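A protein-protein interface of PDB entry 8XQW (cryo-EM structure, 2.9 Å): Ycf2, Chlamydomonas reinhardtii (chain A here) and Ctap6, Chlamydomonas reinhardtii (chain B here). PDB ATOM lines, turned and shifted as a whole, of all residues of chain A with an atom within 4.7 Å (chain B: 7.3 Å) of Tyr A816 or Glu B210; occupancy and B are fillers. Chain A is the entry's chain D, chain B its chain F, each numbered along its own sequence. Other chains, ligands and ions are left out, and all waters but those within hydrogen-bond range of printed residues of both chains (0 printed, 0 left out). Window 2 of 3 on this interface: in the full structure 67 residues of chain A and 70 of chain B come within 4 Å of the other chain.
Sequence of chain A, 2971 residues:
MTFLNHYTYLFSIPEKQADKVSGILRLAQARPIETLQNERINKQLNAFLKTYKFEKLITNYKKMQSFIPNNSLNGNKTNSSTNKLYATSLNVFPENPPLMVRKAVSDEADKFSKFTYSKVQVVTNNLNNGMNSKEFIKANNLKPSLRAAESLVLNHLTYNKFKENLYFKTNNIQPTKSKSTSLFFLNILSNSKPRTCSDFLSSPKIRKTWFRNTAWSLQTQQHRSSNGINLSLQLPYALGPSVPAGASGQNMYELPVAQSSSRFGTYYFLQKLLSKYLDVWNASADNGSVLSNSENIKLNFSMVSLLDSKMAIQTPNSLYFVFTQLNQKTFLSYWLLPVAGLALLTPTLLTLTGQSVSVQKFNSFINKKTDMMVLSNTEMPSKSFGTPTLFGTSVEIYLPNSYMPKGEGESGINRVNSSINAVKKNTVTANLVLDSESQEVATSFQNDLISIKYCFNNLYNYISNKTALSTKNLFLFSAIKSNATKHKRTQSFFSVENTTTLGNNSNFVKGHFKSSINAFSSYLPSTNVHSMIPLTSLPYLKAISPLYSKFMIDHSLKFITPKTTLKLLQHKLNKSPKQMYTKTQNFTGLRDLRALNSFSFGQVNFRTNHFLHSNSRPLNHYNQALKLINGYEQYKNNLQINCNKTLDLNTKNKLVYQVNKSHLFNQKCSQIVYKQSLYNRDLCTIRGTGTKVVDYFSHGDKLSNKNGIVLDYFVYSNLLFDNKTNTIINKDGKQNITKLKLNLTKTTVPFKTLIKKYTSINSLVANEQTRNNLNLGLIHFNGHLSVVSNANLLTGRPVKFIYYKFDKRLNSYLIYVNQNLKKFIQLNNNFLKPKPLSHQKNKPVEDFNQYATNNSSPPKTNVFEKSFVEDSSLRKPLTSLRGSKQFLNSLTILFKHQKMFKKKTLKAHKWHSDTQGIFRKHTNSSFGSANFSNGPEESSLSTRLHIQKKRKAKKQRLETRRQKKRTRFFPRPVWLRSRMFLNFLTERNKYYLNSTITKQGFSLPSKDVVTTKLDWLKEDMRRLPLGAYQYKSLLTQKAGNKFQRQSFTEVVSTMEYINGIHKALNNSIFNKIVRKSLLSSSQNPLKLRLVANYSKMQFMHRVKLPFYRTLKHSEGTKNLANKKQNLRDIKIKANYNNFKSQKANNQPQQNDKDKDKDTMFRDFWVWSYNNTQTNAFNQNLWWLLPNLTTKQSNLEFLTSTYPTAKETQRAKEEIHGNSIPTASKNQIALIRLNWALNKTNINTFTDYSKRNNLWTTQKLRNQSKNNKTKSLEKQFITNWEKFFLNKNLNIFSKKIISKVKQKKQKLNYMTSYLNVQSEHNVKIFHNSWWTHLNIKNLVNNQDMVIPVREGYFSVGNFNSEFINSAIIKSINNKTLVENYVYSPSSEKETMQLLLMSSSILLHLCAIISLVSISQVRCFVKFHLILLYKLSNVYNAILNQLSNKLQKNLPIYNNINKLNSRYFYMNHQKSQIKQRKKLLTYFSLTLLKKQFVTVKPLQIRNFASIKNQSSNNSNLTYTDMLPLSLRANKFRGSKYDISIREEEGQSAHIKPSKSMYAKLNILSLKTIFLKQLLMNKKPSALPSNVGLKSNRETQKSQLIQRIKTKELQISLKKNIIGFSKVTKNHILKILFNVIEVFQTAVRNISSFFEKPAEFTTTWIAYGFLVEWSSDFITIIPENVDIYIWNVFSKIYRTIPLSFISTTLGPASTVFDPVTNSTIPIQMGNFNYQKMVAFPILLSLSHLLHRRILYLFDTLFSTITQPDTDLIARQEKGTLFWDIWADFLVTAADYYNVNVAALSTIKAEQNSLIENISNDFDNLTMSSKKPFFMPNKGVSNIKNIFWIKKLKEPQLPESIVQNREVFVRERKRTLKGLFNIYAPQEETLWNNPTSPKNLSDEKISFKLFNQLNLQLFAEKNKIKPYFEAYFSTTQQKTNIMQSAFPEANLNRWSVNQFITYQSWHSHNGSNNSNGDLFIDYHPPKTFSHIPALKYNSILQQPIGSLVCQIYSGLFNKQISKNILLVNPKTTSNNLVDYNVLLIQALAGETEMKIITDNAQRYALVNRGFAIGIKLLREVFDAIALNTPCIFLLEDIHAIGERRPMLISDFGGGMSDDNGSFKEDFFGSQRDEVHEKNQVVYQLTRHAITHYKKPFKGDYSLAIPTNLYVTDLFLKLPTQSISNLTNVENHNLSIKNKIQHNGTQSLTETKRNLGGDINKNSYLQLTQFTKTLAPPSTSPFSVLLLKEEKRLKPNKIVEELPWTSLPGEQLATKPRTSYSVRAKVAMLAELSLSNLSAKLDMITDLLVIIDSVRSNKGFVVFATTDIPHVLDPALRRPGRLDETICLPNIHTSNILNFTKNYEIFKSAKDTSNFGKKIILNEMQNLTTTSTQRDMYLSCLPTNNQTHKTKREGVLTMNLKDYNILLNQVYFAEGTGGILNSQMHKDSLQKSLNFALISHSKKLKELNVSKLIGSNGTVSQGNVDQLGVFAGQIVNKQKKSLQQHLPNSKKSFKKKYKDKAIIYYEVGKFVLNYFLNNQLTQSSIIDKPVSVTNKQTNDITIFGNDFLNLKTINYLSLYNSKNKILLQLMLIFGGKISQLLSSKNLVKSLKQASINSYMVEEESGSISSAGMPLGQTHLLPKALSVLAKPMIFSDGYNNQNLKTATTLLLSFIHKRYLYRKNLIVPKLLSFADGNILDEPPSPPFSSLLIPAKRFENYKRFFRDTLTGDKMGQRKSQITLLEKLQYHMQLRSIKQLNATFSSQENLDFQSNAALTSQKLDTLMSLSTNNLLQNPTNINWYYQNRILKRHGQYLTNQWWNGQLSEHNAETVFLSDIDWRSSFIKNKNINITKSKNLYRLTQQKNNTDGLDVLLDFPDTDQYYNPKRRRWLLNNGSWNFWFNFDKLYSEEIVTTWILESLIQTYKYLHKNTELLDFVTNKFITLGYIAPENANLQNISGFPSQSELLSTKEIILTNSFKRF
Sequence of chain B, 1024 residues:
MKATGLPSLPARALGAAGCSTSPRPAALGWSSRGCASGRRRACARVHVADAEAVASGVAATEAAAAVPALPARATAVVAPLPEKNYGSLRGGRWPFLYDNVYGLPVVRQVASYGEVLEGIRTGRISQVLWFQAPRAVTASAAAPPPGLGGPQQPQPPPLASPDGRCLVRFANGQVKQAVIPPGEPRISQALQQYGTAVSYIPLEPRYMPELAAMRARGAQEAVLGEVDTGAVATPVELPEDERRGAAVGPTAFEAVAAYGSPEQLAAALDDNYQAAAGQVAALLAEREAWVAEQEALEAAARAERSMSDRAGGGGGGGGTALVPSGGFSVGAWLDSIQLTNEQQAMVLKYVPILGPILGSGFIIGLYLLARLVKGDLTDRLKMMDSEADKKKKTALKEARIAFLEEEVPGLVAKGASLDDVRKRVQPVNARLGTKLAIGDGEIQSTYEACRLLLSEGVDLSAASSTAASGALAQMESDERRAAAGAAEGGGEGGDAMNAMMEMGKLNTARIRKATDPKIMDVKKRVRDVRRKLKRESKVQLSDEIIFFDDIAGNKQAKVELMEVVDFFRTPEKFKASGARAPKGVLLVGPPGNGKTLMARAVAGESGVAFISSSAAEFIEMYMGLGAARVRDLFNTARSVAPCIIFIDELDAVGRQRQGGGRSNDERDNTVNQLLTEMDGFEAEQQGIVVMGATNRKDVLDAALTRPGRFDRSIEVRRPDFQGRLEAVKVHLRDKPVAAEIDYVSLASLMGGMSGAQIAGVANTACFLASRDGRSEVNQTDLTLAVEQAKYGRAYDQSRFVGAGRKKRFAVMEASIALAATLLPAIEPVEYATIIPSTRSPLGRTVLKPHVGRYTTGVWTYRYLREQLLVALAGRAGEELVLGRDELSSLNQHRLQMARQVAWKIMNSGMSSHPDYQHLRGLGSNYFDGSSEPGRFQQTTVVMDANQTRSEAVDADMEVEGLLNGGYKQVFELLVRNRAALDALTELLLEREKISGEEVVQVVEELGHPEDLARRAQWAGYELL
Among the printed residues, pairs that only touch across the chains: Tyr A816 with Glu B210, Tyr A813 with Glu B210, Ser A812 with Gln B155, Ser A812 with Glu B210 and Tyr A813 with Met B214.
ND2 of Asn A820 sits at hydrogen-bond distance from O of Tyr A816, at 3.0 Å.
Tyr A816 touches just one residue of chain B: Glu B210 (3.7 Å). Of chain A, only Ser A812 (3.8 Å), Tyr A813 (3.7 Å) and Tyr A816 (3.7 Å) come within 4 Å of Glu B210. Of the printed residues of chain B, Tyr A813 touches Glu B210 (3.7 Å) and Met B214 (3.8 Å). Of the printed residues of chain B, Ser A812 touches Gln B155 and Glu B210. Of the printed residues of chain A, Gln B155 touches Ser A812. Val A817 touches none of the printed residues of chain B. Met B208 touches none of the printed residues of chain A. The nearest residue of chain B that does not touch Tyr A816 is Leu B211 (4.5 Å). The nearest printed residue of chain B that does not touch Ser A812 is Pro B209 (4.1 Å).
Of the 9 printed residues of chain A, 3 touch a printed residue of chain B. Printed residues of chain A that touch a printed residue of chain B: Ser A812, Tyr A813 and Tyr A816. Printed residues of chain B that touch a printed residue of chain A: Gln B155, Glu B210 and Met B214. Hydrophobic or aromatic side chains of chain B that line the printed part of chain A: Met B214.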
ATOM      1  N   SER A 812     -12.639 -26.445   5.687  1.00  0.00           N
ATOM      2  CA  SER A 812     -12.820 -25.025   5.423  1.00  0.00           C
ATOM      3  C   SER A 812     -13.368 -24.807   4.022  1.00  0.00           C
ATOM      4  O   SER A 812     -14.352 -24.080   3.828  1.00  0.00           O
ATOM      5  CB  SER A 812     -11.495 -24.292   5.596  1.00  0.00           C
ATOM      6  OG  SER A 812     -11.715 -22.908   5.777  1.00  0.00           O
ATOM      7  N   TYR A 813     -12.740 -25.444   3.033  1.00  0.00           N
ATOM      8  CA  TYR A 813     -13.209 -25.333   1.656  1.00  0.00           C
ATOM      9  C   TYR A 813     -14.661 -25.782   1.529  1.00  0.00           C
ATOM     10  O   TYR A 813     -15.490 -25.109   0.897  1.00  0.00           O
ATOM     11  CB  TYR A 813     -12.300 -26.165   0.755  1.00  0.00           C
ATOM     12  CG  TYR A 813     -12.633 -26.090  -0.704  1.00  0.00           C
ATOM     13  CD1 TYR A 813     -12.444 -24.923  -1.417  1.00  0.00           C
ATOM     14  CD2 TYR A 813     -13.139 -27.189  -1.370  1.00  0.00           C
ATOM     15  CE1 TYR A 813     -12.748 -24.854  -2.752  1.00  0.00           C
ATOM     16  CE2 TYR A 813     -13.450 -27.128  -2.705  1.00  0.00           C
ATOM     17  CZ  TYR A 813     -13.253 -25.959  -3.392  1.00  0.00           C
ATOM     18  OH  TYR A 813     -13.563 -25.899  -4.729  1.00  0.00           O
ATOM     19  N   LEU A 814     -14.988 -26.918   2.139  1.00  0.00           N
ATOM     20  CA  LEU A 814     -16.329 -27.472   2.008  1.00  0.00           C
ATOM     21  C   LEU A 814     -17.367 -26.561   2.639  1.00  0.00           C
ATOM     22  O   LEU A 814     -18.440 -26.348   2.066  1.00  0.00           O
ATOM     23  CB  LEU A 814     -16.386 -28.860   2.636  1.00  0.00           C
ATOM     24  CG  LEU A 814     -15.419 -29.896   2.070  1.00  0.00           C
ATOM     25  CD1 LEU A 814     -15.609 -31.236   2.748  1.00  0.00           C
ATOM     26  CD2 LEU A 814     -15.582 -30.018   0.570  1.00  0.00           C
ATOM     27  N   ILE A 815     -17.077 -26.021   3.821  1.00  0.00           N
ATOM     28  CA  ILE A 815     -18.039 -25.142   4.474  1.00  0.00           C
ATOM     29  C   ILE A 815     -18.203 -23.860   3.679  1.00  0.00           C
ATOM     30  O   ILE A 815     -19.302 -23.302   3.596  1.00  0.00           O
ATOM     31  CB  ILE A 815     -17.616 -24.866   5.927  1.00  0.00           C
ATOM     32  CG1 ILE A 815     -17.537 -26.169   6.707  1.00  0.00           C
ATOM     33  CG2 ILE A 815     -18.617 -23.972   6.598  1.00  0.00           C
ATOM     34  CD1 ILE A 815     -16.989 -26.000   8.090  1.00  0.00           C
ATOM     35  N   TYR A 816     -17.123 -23.382   3.064  1.00  0.00           N
ATOM     36  CA  TYR A 816     -17.230 -22.212   2.201  1.00  0.00           C
ATOM     37  C   TYR A 816     -18.220 -22.456   1.072  1.00  0.00           C
ATOM     38  O   TYR A 816     -19.158 -21.670   0.859  1.00  0.00           O
ATOM     39  CB  TYR A 816     -15.855 -21.863   1.644  1.00  0.00           C
ATOM     40  CG  TYR A 816     -15.837 -20.640   0.772  1.00  0.00           C
ATOM     41  CD1 TYR A 816     -16.245 -19.411   1.262  1.00  0.00           C
ATOM     42  CD2 TYR A 816     -15.397 -20.708  -0.537  1.00  0.00           C
ATOM     43  CE1 TYR A 816     -16.220 -18.286   0.472  1.00  0.00           C
ATOM     44  CE2 TYR A 816     -15.370 -19.589  -1.337  1.00  0.00           C
ATOM     45  CZ  TYR A 816     -15.783 -18.380  -0.829  1.00  0.00           C
ATOM     46  OH  TYR A 816     -15.757 -17.258  -1.623  1.00  0.00           O
ATOM     47  N   VAL A 817     -18.035 -23.559   0.345  1.00  0.00           N
ATOM     48  CA  VAL A 817     -18.905 -23.823  -0.798  1.00  0.00           C
ATOM     49  C   VAL A 817     -20.331 -24.112  -0.337  1.00  0.00           C
ATOM     50  O   VAL A 817     -21.297 -23.716  -0.998  1.00  0.00           O
ATOM     51  CB  VAL A 817     -18.335 -24.960  -1.666  1.00  0.00           C
ATOM     52  CG1 VAL A 817     -16.867 -24.714  -1.958  1.00  0.00           C
ATOM     53  CG2 VAL A 817     -18.535 -26.307  -1.013  1.00  0.00           C
ATOM     54  N   ASN A 818     -20.493 -24.767   0.816  1.00  0.00           N
ATOM     55  CA  ASN A 818     -21.835 -25.033   1.319  1.00  0.00           C
ATOM     56  C   ASN A 818     -22.562 -23.744   1.657  1.00  0.00           C
ATOM     57  O   ASN A 818     -23.727 -23.569   1.288  1.00  0.00           O
ATOM     58  CB  ASN A 818     -21.781 -25.927   2.553  1.00  0.00           C
ATOM     59  CG  ASN A 818     -21.264 -27.305   2.249  1.00  0.00           C
ATOM     60  OD1 ASN A 818     -20.966 -28.080   3.156  1.00  0.00           O
ATOM     61  ND2 ASN A 818     -21.143 -27.622   0.969  1.00  0.00           N
ATOM     62  N   GLN A 819     -21.895 -22.841   2.374  1.00  0.00           N
ATOM     63  CA  GLN A 819     -22.516 -21.575   2.740  1.00  0.00           C
ATOM     64  C   GLN A 819     -22.918 -20.790   1.502  1.00  0.00           C
ATOM     65  O   GLN A 819     -24.043 -20.281   1.411  1.00  0.00           O
ATOM     66  CB  GLN A 819     -21.555 -20.769   3.613  1.00  0.00           C
ATOM     67  CG  GLN A 819     -21.902 -19.298   3.741  1.00  0.00           C
ATOM     68  CD  GLN A 819     -20.701 -18.438   4.110  1.00  0.00           C
ATOM     69  OE1 GLN A 819     -20.781 -17.211   4.110  1.00  0.00           O
ATOM     70  NE2 GLN A 819     -19.583 -19.082   4.421  1.00  0.00           N
ATOM     71  N   ASN A 820     -22.015 -20.696   0.521  1.00  0.00           N
ATOM     72  CA  ASN A 820     -22.349 -19.926  -0.672  1.00  0.00           C
ATOM     73  C   ASN A 820     -23.495 -20.562  -1.447  1.00  0.00           C
ATOM     74  O   ASN A 820     -24.403 -19.861  -1.913  1.00  0.00           O
ATOM     75  CB  ASN A 820     -21.125 -19.769  -1.560  1.00  0.00           C
ATOM     76  CG  ASN A 820     -20.240 -18.647  -1.113  1.00  0.00           C
ATOM     77  OD1 ASN A 820     -20.553 -17.476  -1.316  1.00  0.00           O
ATOM     78  ND2 ASN A 820     -19.124 -18.990  -0.492  1.00  0.00           N
ATOM     79  N   PRO B 154     -17.422 -21.353  10.444  1.00  0.00           N
ATOM     80  CA  PRO B 154     -16.945 -21.135   9.076  1.00  0.00           C
ATOM     81  C   PRO B 154     -15.618 -20.406   8.962  1.00  0.00           C
ATOM     82  O   PRO B 154     -14.611 -21.031   8.619  1.00  0.00           O
ATOM     83  CB  PRO B 154     -18.073 -20.304   8.454  1.00  0.00           C
ATOM     84  CG  PRO B 154     -18.769 -19.691   9.605  1.00  0.00           C
ATOM     85  CD  PRO B 154     -18.725 -20.717  10.673  1.00  0.00           C
ATOM     86  N   GLN B 155     -15.587 -19.117   9.292  1.00  0.00           N
ATOM     87  CA  GLN B 155     -14.373 -18.318   9.176  1.00  0.00           C
ATOM     88  C   GLN B 155     -14.627 -16.911   9.695  1.00  0.00           C
ATOM     89  O   GLN B 155     -15.660 -16.313   9.373  1.00  0.00           O
ATOM     90  CB  GLN B 155     -13.889 -18.255   7.728  1.00  0.00           C
ATOM     91  CG  GLN B 155     -12.426 -17.901   7.568  1.00  0.00           C
ATOM     92  CD  GLN B 155     -11.499 -18.978   8.084  1.00  0.00           C
ATOM     93  OE1 GLN B 155     -11.883 -20.135   8.211  1.00  0.00           O
ATOM     94  NE2 GLN B 155     -10.265 -18.600   8.378  1.00  0.00           N
ATOM     95  N   PRO B 156     -13.707 -16.329  10.463  1.00  0.00           N
ATOM     96  CA  PRO B 156     -13.906 -14.961  10.913  1.00  0.00           C
ATOM     97  C   PRO B 156     -13.706 -13.990   9.767  1.00  0.00           C
ATOM     98  O   PRO B 156     -12.983 -14.289   8.801  1.00  0.00           O
ATOM     99  CB  PRO B 156     -12.823 -14.784  11.991  1.00  0.00           C
ATOM    100  CG  PRO B 156     -12.396 -16.158  12.337  1.00  0.00           C
ATOM    101  CD  PRO B 156     -12.537 -16.947  11.095  1.00  0.00           C
ATOM    102  N   PRO B 205      -6.486 -14.748  -3.751  1.00  0.00           N
ATOM    103  CA  PRO B 205      -6.788 -16.164  -3.504  1.00  0.00           C
ATOM    104  C   PRO B 205      -5.661 -16.952  -2.876  1.00  0.00           C
ATOM    105  O   PRO B 205      -5.931 -17.851  -2.074  1.00  0.00           O
ATOM    106  CB  PRO B 205      -7.127 -16.681  -4.904  1.00  0.00           C
ATOM    107  CG  PRO B 205      -7.646 -15.495  -5.597  1.00  0.00           C
ATOM    108  CD  PRO B 205      -6.794 -14.371  -5.135  1.00  0.00           C
ATOM    109  N   TYR B 207      -3.937 -16.144  -0.582  1.00  0.00           N
ATOM    110  CA  TYR B 207      -3.844 -15.740   0.807  1.00  0.00           C
ATOM    111  C   TYR B 207      -5.138 -15.921   1.578  1.00  0.00           C
ATOM    112  O   TYR B 207      -5.110 -15.861   2.809  1.00  0.00           O
ATOM    113  CB  TYR B 207      -3.406 -14.275   0.907  1.00  0.00           C
ATOM    114  CG  TYR B 207      -1.939 -14.080   0.659  1.00  0.00           C
ATOM    115  CD1 TYR B 207      -1.028 -15.052   1.014  1.00  0.00           C
ATOM    116  CD2 TYR B 207      -1.465 -12.932   0.062  1.00  0.00           C
ATOM    117  CE1 TYR B 207       0.312 -14.884   0.792  1.00  0.00           C
ATOM    118  CE2 TYR B 207      -0.126 -12.754  -0.166  1.00  0.00           C
ATOM    119  CZ  TYR B 207       0.758 -13.734   0.204  1.00  0.00           C
ATOM    120  OH  TYR B 207       2.100 -13.569  -0.019  1.00  0.00           O
ATOM    121  N   MET B 208      -6.261 -16.125   0.904  1.00  0.00           N
ATOM    122  CA  MET B 208      -7.485 -16.454   1.612  1.00  0.00           C
ATOM    123  C   MET B 208      -7.304 -17.782   2.337  1.00  0.00           C
ATOM    124  O   MET B 208      -6.670 -18.697   1.805  1.00  0.00           O
ATOM    125  CB  MET B 208      -8.661 -16.542   0.644  1.00  0.00           C
ATOM    126  CG  MET B 208      -9.004 -15.230  -0.009  1.00  0.00           C
ATOM    127  SD  MET B 208     -10.432 -15.349  -1.090  1.00  0.00           S
ATOM    128  CE  MET B 208     -11.694 -15.780   0.090  1.00  0.00           C
ATOM    129  N   PRO B 209      -7.832 -17.923   3.554  1.00  0.00           N
ATOM    130  CA  PRO B 209      -7.617 -19.160   4.311  1.00  0.00           C
ATOM    131  C   PRO B 209      -8.492 -20.313   3.867  1.00  0.00           C
ATOM    132  O   PRO B 209      -8.181 -21.460   4.209  1.00  0.00           O
ATOM    133  CB  PRO B 209      -7.949 -18.753   5.751  1.00  0.00           C
ATOM    134  CG  PRO B 209      -8.125 -17.271   5.724  1.00  0.00           C
ATOM    135  CD  PRO B 209      -8.554 -16.926   4.350  1.00  0.00           C
ATOM    136  N   GLU B 210      -9.568 -20.061   3.130  1.00  0.00           N
ATOM    137  CA  GLU B 210     -10.456 -21.128   2.702  1.00  0.00           C
ATOM    138  C   GLU B 210      -9.996 -21.821   1.429  1.00  0.00           C
ATOM    139  O   GLU B 210     -10.505 -22.899   1.115  1.00  0.00           O
ATOM    140  CB  GLU B 210     -11.864 -20.586   2.488  1.00  0.00           C
ATOM    141  CG  GLU B 210     -12.353 -19.714   3.610  1.00  0.00           C
ATOM    142  CD  GLU B 210     -13.118 -18.521   3.100  1.00  0.00           C
ATOM    143  OE1 GLU B 210     -14.005 -18.023   3.821  1.00  0.00           O
ATOM    144  OE2 GLU B 210     -12.830 -18.083   1.969  1.00  0.00           O
ATOM    145  N   LEU B 211      -9.056 -21.237   0.694  1.00  0.00           N
ATOM    146  CA  LEU B 211      -8.564 -21.830  -0.542  1.00  0.00           C
ATOM    147  C   LEU B 211      -7.130 -22.318  -0.409  1.00  0.00           C
ATOM    148  O   LEU B 211      -6.463 -22.543  -1.419  1.00  0.00           O
ATOM    149  CB  LEU B 211      -8.680 -20.836  -1.694  1.00  0.00           C
ATOM    150  CG  LEU B 211     -10.030 -20.139  -1.780  1.00  0.00           C
ATOM    151  CD1 LEU B 211     -10.042 -19.166  -2.931  1.00  0.00           C
ATOM    152  CD2 LEU B 211     -11.140 -21.155  -1.923  1.00  0.00           C
ATOM    153  N   ALA B 212      -6.637 -22.480   0.817  1.00  0.00           N
ATOM    154  CA  ALA B 212      -5.303 -23.040   0.990  1.00  0.00           C
ATOM    155  C   ALA B 212      -5.244 -24.483   0.518  1.00  0.00           C
ATOM    156  O   ALA B 212      -4.193 -24.945   0.062  1.00  0.00           O
ATOM    157  CB  ALA B 212      -4.876 -22.942   2.450  1.00  0.00           C
ATOM    158  N   ALA B 213      -6.358 -25.211   0.615  1.00  0.00           N
ATOM    159  CA  ALA B 213      -6.401 -26.568   0.086  1.00  0.00           C
ATOM    160  C   ALA B 213      -6.197 -26.567  -1.423  1.00  0.00           C
ATOM    161  O   ALA B 213      -5.434 -27.378  -1.959  1.00  0.00           O
ATOM    162  CB  ALA B 213      -7.726 -27.230   0.451  1.00  0.00           C
ATOM    163  N   MET B 214      -6.871 -25.655  -2.125  1.00  0.00           N
ATOM    164  CA  MET B 214      -6.688 -25.551  -3.567  1.00  0.00           C
ATOM    165  C   MET B 214      -5.274 -25.124  -3.924  1.00  0.00           C
ATOM    166  O   MET B 214      -4.690 -25.652  -4.875  1.00  0.00           O
ATOM    167  CB  MET B 214      -7.700 -24.573  -4.153  1.00  0.00           C
ATOM    168  CG  MET B 214      -9.134 -25.004  -3.971  1.00  0.00           C
ATOM    169  SD  MET B 214      -9.473 -26.605  -4.722  1.00  0.00           S
ATOM    170  CE  MET B 214      -9.597 -27.639  -3.268  1.00  0.00           C
